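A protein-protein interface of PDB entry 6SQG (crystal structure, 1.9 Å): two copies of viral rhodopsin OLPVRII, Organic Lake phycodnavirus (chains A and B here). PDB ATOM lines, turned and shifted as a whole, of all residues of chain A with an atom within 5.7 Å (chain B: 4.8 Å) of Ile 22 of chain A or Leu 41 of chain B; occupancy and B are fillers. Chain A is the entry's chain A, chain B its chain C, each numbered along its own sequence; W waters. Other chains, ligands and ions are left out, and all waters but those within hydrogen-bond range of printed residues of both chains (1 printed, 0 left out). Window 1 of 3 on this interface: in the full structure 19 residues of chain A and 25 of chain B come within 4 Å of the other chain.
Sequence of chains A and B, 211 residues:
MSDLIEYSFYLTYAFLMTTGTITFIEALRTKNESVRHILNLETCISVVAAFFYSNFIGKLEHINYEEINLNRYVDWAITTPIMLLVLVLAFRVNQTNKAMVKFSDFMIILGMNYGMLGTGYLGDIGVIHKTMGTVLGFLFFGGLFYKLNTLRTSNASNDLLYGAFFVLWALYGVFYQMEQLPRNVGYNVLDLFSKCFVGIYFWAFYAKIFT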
ATOM      1  N   MET A  17     -26.305 -31.093  16.451  1.00  0.00           N
ATOM      2  CA  MET A  17     -24.933 -31.108  16.960  1.00  0.00           C
ATOM      3  C   MET A  17     -24.568 -29.748  17.538  1.00  0.00           C
ATOM      4  O   MET A  17     -23.940 -29.663  18.583  1.00  0.00           O
ATOM      5  CB  MET A  17     -23.945 -31.456  15.853  1.00  0.00           C
ATOM      6  CG  MET A  17     -24.115 -32.847  15.274  1.00  0.00           C
ATOM      7  SD  MET A  17     -22.884 -33.189  13.997  1.00  0.00           S
ATOM      8  CE  MET A  17     -23.748 -34.471  13.089  1.00  0.00           C
ATOM      9  N   THR A  18     -24.963 -28.691  16.844  1.00  0.00           N
ATOM     10  CA  THR A  18     -24.702 -27.333  17.280  1.00  0.00           C
ATOM     11  C   THR A  18     -25.381 -27.045  18.601  1.00  0.00           C
ATOM     12  O   THR A  18     -24.755 -26.564  19.546  1.00  0.00           O
ATOM     13  CB  THR A  18     -25.216 -26.323  16.232  1.00  0.00           C
ATOM     14  OG1 THR A  18     -24.444 -26.458  15.035  1.00  0.00           O
ATOM     15  CG2 THR A  18     -25.091 -24.899  16.743  1.00  0.00           C
ATOM     16  N   THR A  19     -26.671 -27.347  18.656  1.00  0.00           N
ATOM     17  CA  THR A  19     -27.472 -27.046  19.815  1.00  0.00           C
ATOM     18  C   THR A  19     -26.947 -27.833  21.007  1.00  0.00           C
ATOM     19  O   THR A  19     -26.778 -27.285  22.096  1.00  0.00           O
ATOM     20  CB  THR A  19     -28.964 -27.347  19.550  1.00  0.00           C
ATOM     21  OG1 THR A  19     -29.386 -26.619  18.394  1.00  0.00           O
ATOM     22  CG2 THR A  19     -29.842 -26.941  20.753  1.00  0.00           C
ATOM     23  N   GLY A  20     -26.648 -29.106  20.786  1.00  0.00           N
ATOM     24  CA  GLY A  20     -26.126 -29.964  21.848  1.00  0.00           C
ATOM     25  C   GLY A  20     -24.803 -29.480  22.401  1.00  0.00           C
ATOM     26  O   GLY A  20     -24.563 -29.530  23.609  1.00  0.00           O
ATOM     27  N   THR A  21     -23.931 -29.014  21.521  1.00  0.00           N
ATOM     28  CA  THR A  21     -22.634 -28.510  21.947  1.00  0.00           C
ATOM     29  C   THR A  21     -22.812 -27.227  22.763  1.00  0.00           C
ATOM     30  O   THR A  21     -22.210 -27.051  23.821  1.00  0.00           O
ATOM     31  CB  THR A  21     -21.725 -28.229  20.733  1.00  0.00           C
ATOM     32  OG1 THR A  21     -21.552 -29.431  19.963  1.00  0.00           O
ATOM     33  CG2 THR A  21     -20.371 -27.714  21.189  1.00  0.00           C
ATOM     34  N   ILE A  22     -23.657 -26.325  22.297  1.00  0.00           N
ATOM     35  CA  ILE A  22     -23.796 -25.041  22.963  1.00  0.00           C
ATOM     36  C   ILE A  22     -24.361 -25.219  24.379  1.00  0.00           C
ATOM     37  O   ILE A  22     -23.822 -24.665  25.353  1.00  0.00           O
ATOM     38  CB  ILE A  22     -24.631 -24.052  22.109  1.00  0.00           C
ATOM     39  CG1 ILE A  22     -24.172 -22.616  22.359  1.00  0.00           C
ATOM     40  CG2 ILE A  22     -26.123 -24.191  22.375  1.00  0.00           C
ATOM     41  CD1 ILE A  22     -23.247 -22.079  21.300  1.00  0.00           C
ATOM     42  N   THR A  23     -25.421 -26.006  24.504  1.00  0.00           N
ATOM     43  CA  THR A  23     -26.044 -26.219  25.806  1.00  0.00           C
ATOM     44  C   THR A  23     -25.151 -27.045  26.756  1.00  0.00           C
ATOM     45  O   THR A  23     -25.124 -26.805  27.963  1.00  0.00           O
ATOM     46  CB  THR A  23     -27.448 -26.857  25.662  1.00  0.00           C
ATOM     47  OG1 THR A  23     -27.362 -28.134  25.006  1.00  0.00           O
ATOM     48  CG2 THR A  23     -28.357 -25.946  24.860  1.00  0.00           C
ATOM     49  N   PHE A  24     -24.424 -28.015  26.213  1.00  0.00           N
ATOM     50  CA  PHE A  24     -23.491 -28.816  27.012  1.00  0.00           C
ATOM     51  C   PHE A  24     -22.419 -27.954  27.667  1.00  0.00           C
ATOM     52  O   PHE A  24     -22.174 -28.048  28.866  1.00  0.00           O
ATOM     53  CB  PHE A  24     -22.828 -29.849  26.114  1.00  0.00           C
ATOM     54  CG  PHE A  24     -21.803 -30.716  26.801  1.00  0.00           C
ATOM     55  CD1 PHE A  24     -22.184 -31.668  27.737  1.00  0.00           C
ATOM     56  CD2 PHE A  24     -20.469 -30.637  26.442  1.00  0.00           C
ATOM     57  CE1 PHE A  24     -21.239 -32.499  28.329  1.00  0.00           C
ATOM     58  CE2 PHE A  24     -19.524 -31.464  27.021  1.00  0.00           C
ATOM     59  CZ  PHE A  24     -19.910 -32.400  27.960  1.00  0.00           C
ATOM     60  N   ILE A  25     -21.769 -27.115  26.868  1.00  0.00           N
ATOM     61  CA  ILE A  25     -20.714 -26.266  27.385  1.00  0.00           C
ATOM     62  C   ILE A  25     -21.273 -25.300  28.434  1.00  0.00           C
ATOM     63  O   ILE A  25     -20.693 -25.143  29.512  1.00  0.00           O
ATOM     64  CB  ILE A  25     -19.982 -25.516  26.249  1.00  0.00           C
ATOM     65  CG1 ILE A  25     -19.186 -26.506  25.397  1.00  0.00           C
ATOM     66  CG2 ILE A  25     -19.072 -24.446  26.832  1.00  0.00           C
ATOM     67  CD1 ILE A  25     -18.648 -25.936  24.102  1.00  0.00           C
ATOM     68  N   GLU A  26     -22.409 -24.668  28.148  1.00  0.00           N
ATOM     69  CA  GLU A  26     -22.979 -23.739  29.122  1.00  0.00           C
ATOM     70  C   GLU A  26     -23.532 -24.468  30.361  1.00  0.00           C
ATOM     71  O   GLU A  26     -23.463 -23.926  31.457  1.00  0.00           O
ATOM     72  CB  GLU A  26     -24.038 -22.828  28.505  1.00  0.00           C
ATOM     73  CG  GLU A  26     -24.429 -21.652  29.402  1.00  0.00           C
ATOM     74  CD  GLU A  26     -23.243 -20.800  29.847  1.00  0.00           C
ATOM     75  OE1 GLU A  26     -22.161 -20.888  29.229  1.00  0.00           O
ATOM     76  OE2 GLU A  26     -23.388 -20.034  30.818  1.00  0.00           O
ATOM     77  N   ALA A  27     -24.054 -25.685  30.208  1.00  0.00           N
ATOM     78  CA  ALA A  27     -24.493 -26.459  31.403  1.00  0.00           C
ATOM     79  C   ALA A  27     -23.333 -26.666  32.373  1.00  0.00           C
ATOM     80  O   ALA A  27     -23.508 -26.664  33.591  1.00  0.00           O
ATOM     81  CB  ALA A  27     -25.092 -27.802  31.014  1.00  0.00           C
ATOM     82  N   GLY A 199     -33.707 -24.590  21.695  1.00  0.00           N
ATOM     83  CA  GLY A 199     -32.550 -24.846  22.537  1.00  0.00           C
ATOM     84  C   GLY A 199     -31.565 -23.693  22.482  1.00  0.00           C
ATOM     85  O   GLY A 199     -31.034 -23.277  23.499  1.00  0.00           O
ATOM     86  N   ILE A 200     -31.311 -23.171  21.289  1.00  0.00           N
ATOM     87  CA  ILE A 200     -30.433 -22.002  21.164  1.00  0.00           C
ATOM     88  C   ILE A 200     -31.039 -20.784  21.882  1.00  0.00           C
ATOM     89  O   ILE A 200     -30.316 -19.987  22.498  1.00  0.00           O
ATOM     90  CB  ILE A 200     -30.130 -21.703  19.692  1.00  0.00           C
ATOM     91  CG1 ILE A 200     -29.238 -22.810  19.126  1.00  0.00           C
ATOM     92  CG2 ILE A 200     -29.447 -20.356  19.541  1.00  0.00           C
ATOM     93  CD1 ILE A 200     -29.274 -22.912  17.621  1.00  0.00           C
ATOM     94  N   TRP A 203     -30.297 -21.097  25.601  1.00  0.00           N
ATOM     95  CA  TRP A 203     -28.905 -20.739  25.793  1.00  0.00           C
ATOM     96  C   TRP A 203     -28.736 -19.226  25.743  1.00  0.00           C
ATOM     97  O   TRP A 203     -28.176 -18.620  26.657  1.00  0.00           O
ATOM     98  CB  TRP A 203     -28.030 -21.379  24.727  1.00  0.00           C
ATOM     99  CG  TRP A 203     -26.655 -20.865  24.785  1.00  0.00           C
ATOM    100  CD1 TRP A 203     -25.705 -21.175  25.714  1.00  0.00           C
ATOM    101  CD2 TRP A 203     -26.069 -19.891  23.916  1.00  0.00           C
ATOM    102  NE1 TRP A 203     -24.548 -20.465  25.458  1.00  0.00           N
ATOM    103  CE2 TRP A 203     -24.750 -19.674  24.358  1.00  0.00           C
ATOM    104  CE3 TRP A 203     -26.528 -19.192  22.796  1.00  0.00           C
ATOM    105  CZ2 TRP A 203     -23.888 -18.786  23.719  1.00  0.00           C
ATOM    106  CZ3 TRP A 203     -25.671 -18.312  22.167  1.00  0.00           C
ATOM    107  CH2 TRP A 203     -24.364 -18.120  22.629  1.00  0.00           C
ATOM    108  N   HIS B  37     -18.869 -17.470  25.843  1.00  0.00           N
ATOM    109  CA  HIS B  37     -19.948 -17.553  24.872  1.00  0.00           C
ATOM    110  C   HIS B  37     -19.405 -17.545  23.464  1.00  0.00           C
ATOM    111  O   HIS B  37     -19.875 -18.293  22.601  1.00  0.00           O
ATOM    112  CB  HIS B  37     -20.959 -16.426  25.078  1.00  0.00           C
ATOM    113  CG  HIS B  37     -21.549 -16.418  26.447  1.00  0.00           C
ATOM    114  ND1 HIS B  37     -21.800 -17.579  27.147  1.00  0.00           N
ATOM    115  CD2 HIS B  37     -21.936 -15.401  27.252  1.00  0.00           C
ATOM    116  CE1 HIS B  37     -22.307 -17.276  28.329  1.00  0.00           C
ATOM    117  NE2 HIS B  37     -22.395 -15.962  28.419  1.00  0.00           N
ATOM    118  N   ILE B  38     -18.414 -16.695  23.233  1.00  0.00           N
ATOM    119  CA  ILE B  38     -17.783 -16.588  21.930  1.00  0.00           C
ATOM    120  C   ILE B  38     -17.027 -17.867  21.558  1.00  0.00           C
ATOM    121  O   ILE B  38     -17.139 -18.365  20.445  1.00  0.00           O
ATOM    122  CB  ILE B  38     -16.821 -15.388  21.899  1.00  0.00           C
ATOM    123  CG1 ILE B  38     -17.632 -14.087  21.823  1.00  0.00           C
ATOM    124  CG2 ILE B  38     -15.870 -15.495  20.721  1.00  0.00           C
ATOM    125  CD1 ILE B  38     -16.795 -12.842  21.999  1.00  0.00           C
ATOM    126  N   LEU B  39     -16.262 -18.405  22.490  1.00  0.00           N
ATOM    127  CA  LEU B  39     -15.517 -19.630  22.212  1.00  0.00           C
ATOM    128  C   LEU B  39     -16.424 -20.859  22.092  1.00  0.00           C
ATOM    129  O   LEU B  39     -16.104 -21.798  21.362  1.00  0.00           O
ATOM    130  CB  LEU B  39     -14.454 -19.853  23.287  1.00  0.00           C
ATOM    131  CG  LEU B  39     -13.328 -18.819  23.302  1.00  0.00           C
ATOM    132  CD1 LEU B  39     -12.343 -19.163  24.409  1.00  0.00           C
ATOM    133  CD2 LEU B  39     -12.618 -18.749  21.960  1.00  0.00           C
ATOM    134  N   ASN B  40     -17.531 -20.859  22.831  1.00  0.00           N
ATOM    135  CA  ASN B  40     -18.567 -21.875  22.694  1.00  0.00           C
ATOM    136  C   ASN B  40     -19.120 -21.906  21.260  1.00  0.00           C
ATOM    137  O   ASN B  40     -19.112 -22.938  20.599  1.00  0.00           O
ATOM    138  CB  ASN B  40     -19.691 -21.563  23.668  1.00  0.00           C
ATOM    139  CG  ASN B  40     -20.720 -22.674  23.773  1.00  0.00           C
ATOM    140  OD1 ASN B  40     -20.726 -23.627  22.985  1.00  0.00           O
ATOM    141  ND2 ASN B  40     -21.619 -22.539  24.742  1.00  0.00           N
ATOM    142  N   LEU B  41     -19.562 -20.748  20.781  1.00  0.00           N
ATOM    143  CA  LEU B  41     -20.003 -20.611  19.399  1.00  0.00           C
ATOM    144  C   LEU B  41     -18.929 -21.038  18.401  1.00  0.00           C
ATOM    145  O   LEU B  41     -19.229 -21.711  17.418  1.00  0.00           O
ATOM    146  CB  LEU B  41     -20.410 -19.167  19.125  1.00  0.00           C
ATOM    147  CG  LEU B  41     -21.696 -18.726  19.826  1.00  0.00           C
ATOM    148  CD1 LEU B  41     -21.875 -17.216  19.713  1.00  0.00           C
ATOM    149  CD2 LEU B  41     -22.910 -19.465  19.272  1.00  0.00           C
ATOM    150  N   GLU B  42     -17.687 -20.604  18.627  1.00  0.00           N
ATOM    151  CA  GLU B  42     -16.576 -21.002  17.769  1.00  0.00           C
ATOM    152  C   GLU B  42     -16.382 -22.527  17.742  1.00  0.00           C
ATOM    153  O   GLU B  42     -16.121 -23.101  16.697  1.00  0.00           O
ATOM    154  CB  GLU B  42     -15.290 -20.312  18.194  1.00  0.00           C
ATOM    155  CG  GLU B  42     -15.157 -18.888  17.673  1.00  0.00           C
ATOM    156  CD  GLU B  42     -15.075 -18.824  16.157  1.00  0.00           C
ATOM    157  OE1 GLU B  42     -14.347 -19.642  15.556  1.00  0.00           O
ATOM    158  OE2 GLU B  42     -15.741 -17.953  15.559  1.00  0.00           O
ATOM    159  N   THR B  43     -16.510 -23.175  18.889  1.00  0.00           N
ATOM    160  CA  THR B  43     -16.451 -24.632  18.924  1.00  0.00           C
ATOM    161  C   THR B  43     -17.528 -25.262  18.012  1.00  0.00           C
ATOM    162  O   THR B  43     -17.247 -26.202  17.282  1.00  0.00           O
ATOM    163  CB  THR B  43     -16.593 -25.137  20.362  1.00  0.00           C
ATOM    164  OG1 THR B  43     -15.584 -24.505  21.172  1.00  0.00           O
ATOM    165  CG2 THR B  43     -16.425 -26.639  20.413  1.00  0.00           C
ATOM    166  N   CYS B  44     -18.746 -24.733  18.056  1.00  0.00           N
ATOM    167  CA  CYS B  44     -19.842 -25.233  17.230  1.00  0.00           C
ATOM    168  C   CYS B  44     -19.517 -25.135  15.758  1.00  0.00           C
ATOM    169  O   CYS B  44     -19.807 -26.053  14.973  1.00  0.00           O
ATOM    170  CB  CYS B  44     -21.120 -24.437  17.510  1.00  0.00           C
ATOM    171  SG  CYS B  44     -21.768 -24.710  19.165  1.00  0.00           S
ATOM    172  N   ILE B  45     -18.928 -24.006  15.373  1.00  0.00           N
ATOM    173  CA  ILE B  45     -18.545 -23.812  13.984  1.00  0.00           C
ATOM    174  C   ILE B  45     -17.620 -24.926  13.521  1.00  0.00           C
ATOM    175  O   ILE B  45     -17.844 -25.514  12.466  1.00  0.00           O
ATOM    176  CB  ILE B  45     -17.885 -22.459  13.764  1.00  0.00           C
ATOM    177  CG1 ILE B  45     -18.928 -21.350  13.897  1.00  0.00           C
ATOM    178  CG2 ILE B  45     -17.233 -22.394  12.391  1.00  0.00           C
ATOM    179  CD1 ILE B  45     -18.317 -20.003  14.198  1.00  0.00           C
ATOM    180  N   ILE B  82     -23.662 -18.501  12.713  1.00  0.00           N
ATOM    181  CA  ILE B  82     -22.919 -18.614  13.972  1.00  0.00           C
ATOM    182  C   ILE B  82     -21.673 -17.742  13.890  1.00  0.00           C
ATOM    183  O   ILE B  82     -21.338 -17.037  14.846  1.00  0.00           O
ATOM    184  CB  ILE B  82     -22.500 -20.072  14.277  1.00  0.00           C
ATOM    185  CG1 ILE B  82     -23.699 -21.019  14.249  1.00  0.00           C
ATOM    186  CG2 ILE B  82     -21.842 -20.166  15.645  1.00  0.00           C
ATOM    187  CD1 ILE B  82     -23.310 -22.478  14.349  1.00  0.00           C
ATOM    188  N   LEU B  85     -22.741 -14.198  14.311  1.00  0.00           N
ATOM    189  CA  LEU B  85     -23.072 -13.928  15.686  1.00  0.00           C
ATOM    190  C   LEU B  85     -21.793 -13.703  16.489  1.00  0.00           C
ATOM    191  O   LEU B  85     -21.701 -12.749  17.264  1.00  0.00           O
ATOM    192  CB  LEU B  85     -23.917 -15.054  16.289  1.00  0.00           C
ATOM    193  CG  LEU B  85     -24.308 -14.829  17.752  1.00  0.00           C
ATOM    194  CD1 LEU B  85     -25.132 -13.547  17.907  1.00  0.00           C
ATOM    195  CD2 LEU B  85     -25.076 -16.027  18.282  1.00  0.00           C
ATOM    196  N   VAL B  86     -20.804 -14.573  16.299  1.00  0.00           N
ATOM    197  CA  VAL B  86     -19.509 -14.411  16.959  1.00  0.00           C
ATOM    198  C   VAL B  86     -18.908 -13.047  16.645  1.00  0.00           C
ATOM    199  O   VAL B  86     -18.410 -12.347  17.538  1.00  0.00           O
ATOM    200  CB  VAL B  86     -18.504 -15.481  16.505  1.00  0.00           C
ATOM    201  CG1 VAL B  86     -17.077 -15.047  16.818  1.00  0.00           C
ATOM    202  CG2 VAL B  86     -18.805 -16.812  17.178  1.00  0.00           C
ATOM    203  N   LEU B  89     -20.795 -10.199  18.478  1.00  0.00           N
ATOM    204  CA  LEU B  89     -20.523 -10.328  19.898  1.00  0.00           C
ATOM    205  C   LEU B  89     -19.087  -9.914  20.221  1.00  0.00           C
ATOM    206  O   LEU B  89     -18.829  -9.262  21.237  1.00  0.00           O
ATOM    207  CB  LEU B  89     -20.787 -11.752  20.383  1.00  0.00           C
ATOM    208  CG  LEU B  89     -22.243 -12.243  20.346  1.00  0.00           C
ATOM    209  CD1 LEU B  89     -22.296 -13.656  20.894  1.00  0.00           C
ATOM    210  CD2 LEU B  89     -23.189 -11.328  21.107  1.00  0.00           C
HETATM  211  O   HOH W   1     -21.803 -20.338  26.571  1.00  0.00           O
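Printed residues of chain B within 4 Å of Ile 22 of chain A: Asn 40 (3.1 Å), Leu 41 (3.3 Å) and Cys 44 (3.7 Å).
Of the printed residues of chain A, Leu 41 of chain B touches Ile 22 and Trp 203.
Of the printed residues of chain A, Cys 44 of chain B touches Thr 18 (3.5 Å), Thr 21 (3.9 Å) and Ile 22 (3.7 Å).
Printed residues of chain A within 4 Å of Ile 82 of chain B: Thr 18 (3.8 Å).
Printed residues of chain A within 4 Å of Asn 40 of chain B: Thr 21, Ile 22, Ile 25 and Trp 203.
The nearest printed residue of chain B that does not touch Ile 22 of chain A is His 37 of chain B (5.2 Å).
The nearest printed residue of chain A that does not touch Leu 41 of chain B is Ile 25 of chain A (6.2 Å).
The nearest printed residue of chain A that does not touch Asn 40 of chain B is Glu 26 of chain A (4.1 Å).
No position is printed for both chains.
O of Met 17 of chain A is in hydrogen-bond range of OG1 of Thr 21 of chain A, at 2.8 Å.
The side-chain sulfur (SG) of Cys 44 of chain B is in hydrogen-bond range of the backbone carbonyl oxygen (O) of Asn 40 of chain B, 3.5 Å away.
Hydrophobic or aromatic side chains of chain B that line the printed part of chain A: His 37, Leu 41 and Ile 82.
Among the printed residues, 12 pairs touch across the chains.
Water W1 lies within hydrogen-bond range of the side-chain carboxylate of Glu 26 of chain A (2.7 Å), a ring nitrogen (ND1) of His 37 of chain B (2.8 Å), the side-chain amide nitrogen of Asn 40 of chain B (2.9 Å) and the indole nitrogen of Trp 203 of chain A (3.0 Å).
Thr 18 of chain A touches Ile 82 of chain B (CG2 to CD1, 3.8 Å).
O of Thr 21 of chain A touches OD1 of Asn 40 of chain B (3.8 Å).
CB of Thr 21 of chain A touches SG of Cys 44 of chain B, at 3.9 Å.
Ile 22 of chain A touches Leu 41 of chain B.
SG of Cys 44 of chain B touches CD1 of Ile 22 of chain A, 3.7 Å away.
Ile 25 of chain A touches Asn 40 of chain B.
Glu 26 of chain A touches His 37 of chain B.
His 37 of chain B touches Trp 203 of chain A (CB to CZ2, 3.999 Å).
Trp 203 of chain A touches Asn 40 of chain B.
Trp 203 of chain A touches Leu 41 of chain B.
The side-chain amide nitrogen (ND2) of Asn 40 of chain B sits at hydrogen-bond distance from the backbone carbonyl oxygen (O) of Ile 22 of chain A (3.1 Å).
The backbone carbonyl oxygen (O) of Thr 18 of chain A is in hydrogen-bond range of the side-chain sulfur (SG) of Cys 44 of chain B (3.5 Å).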
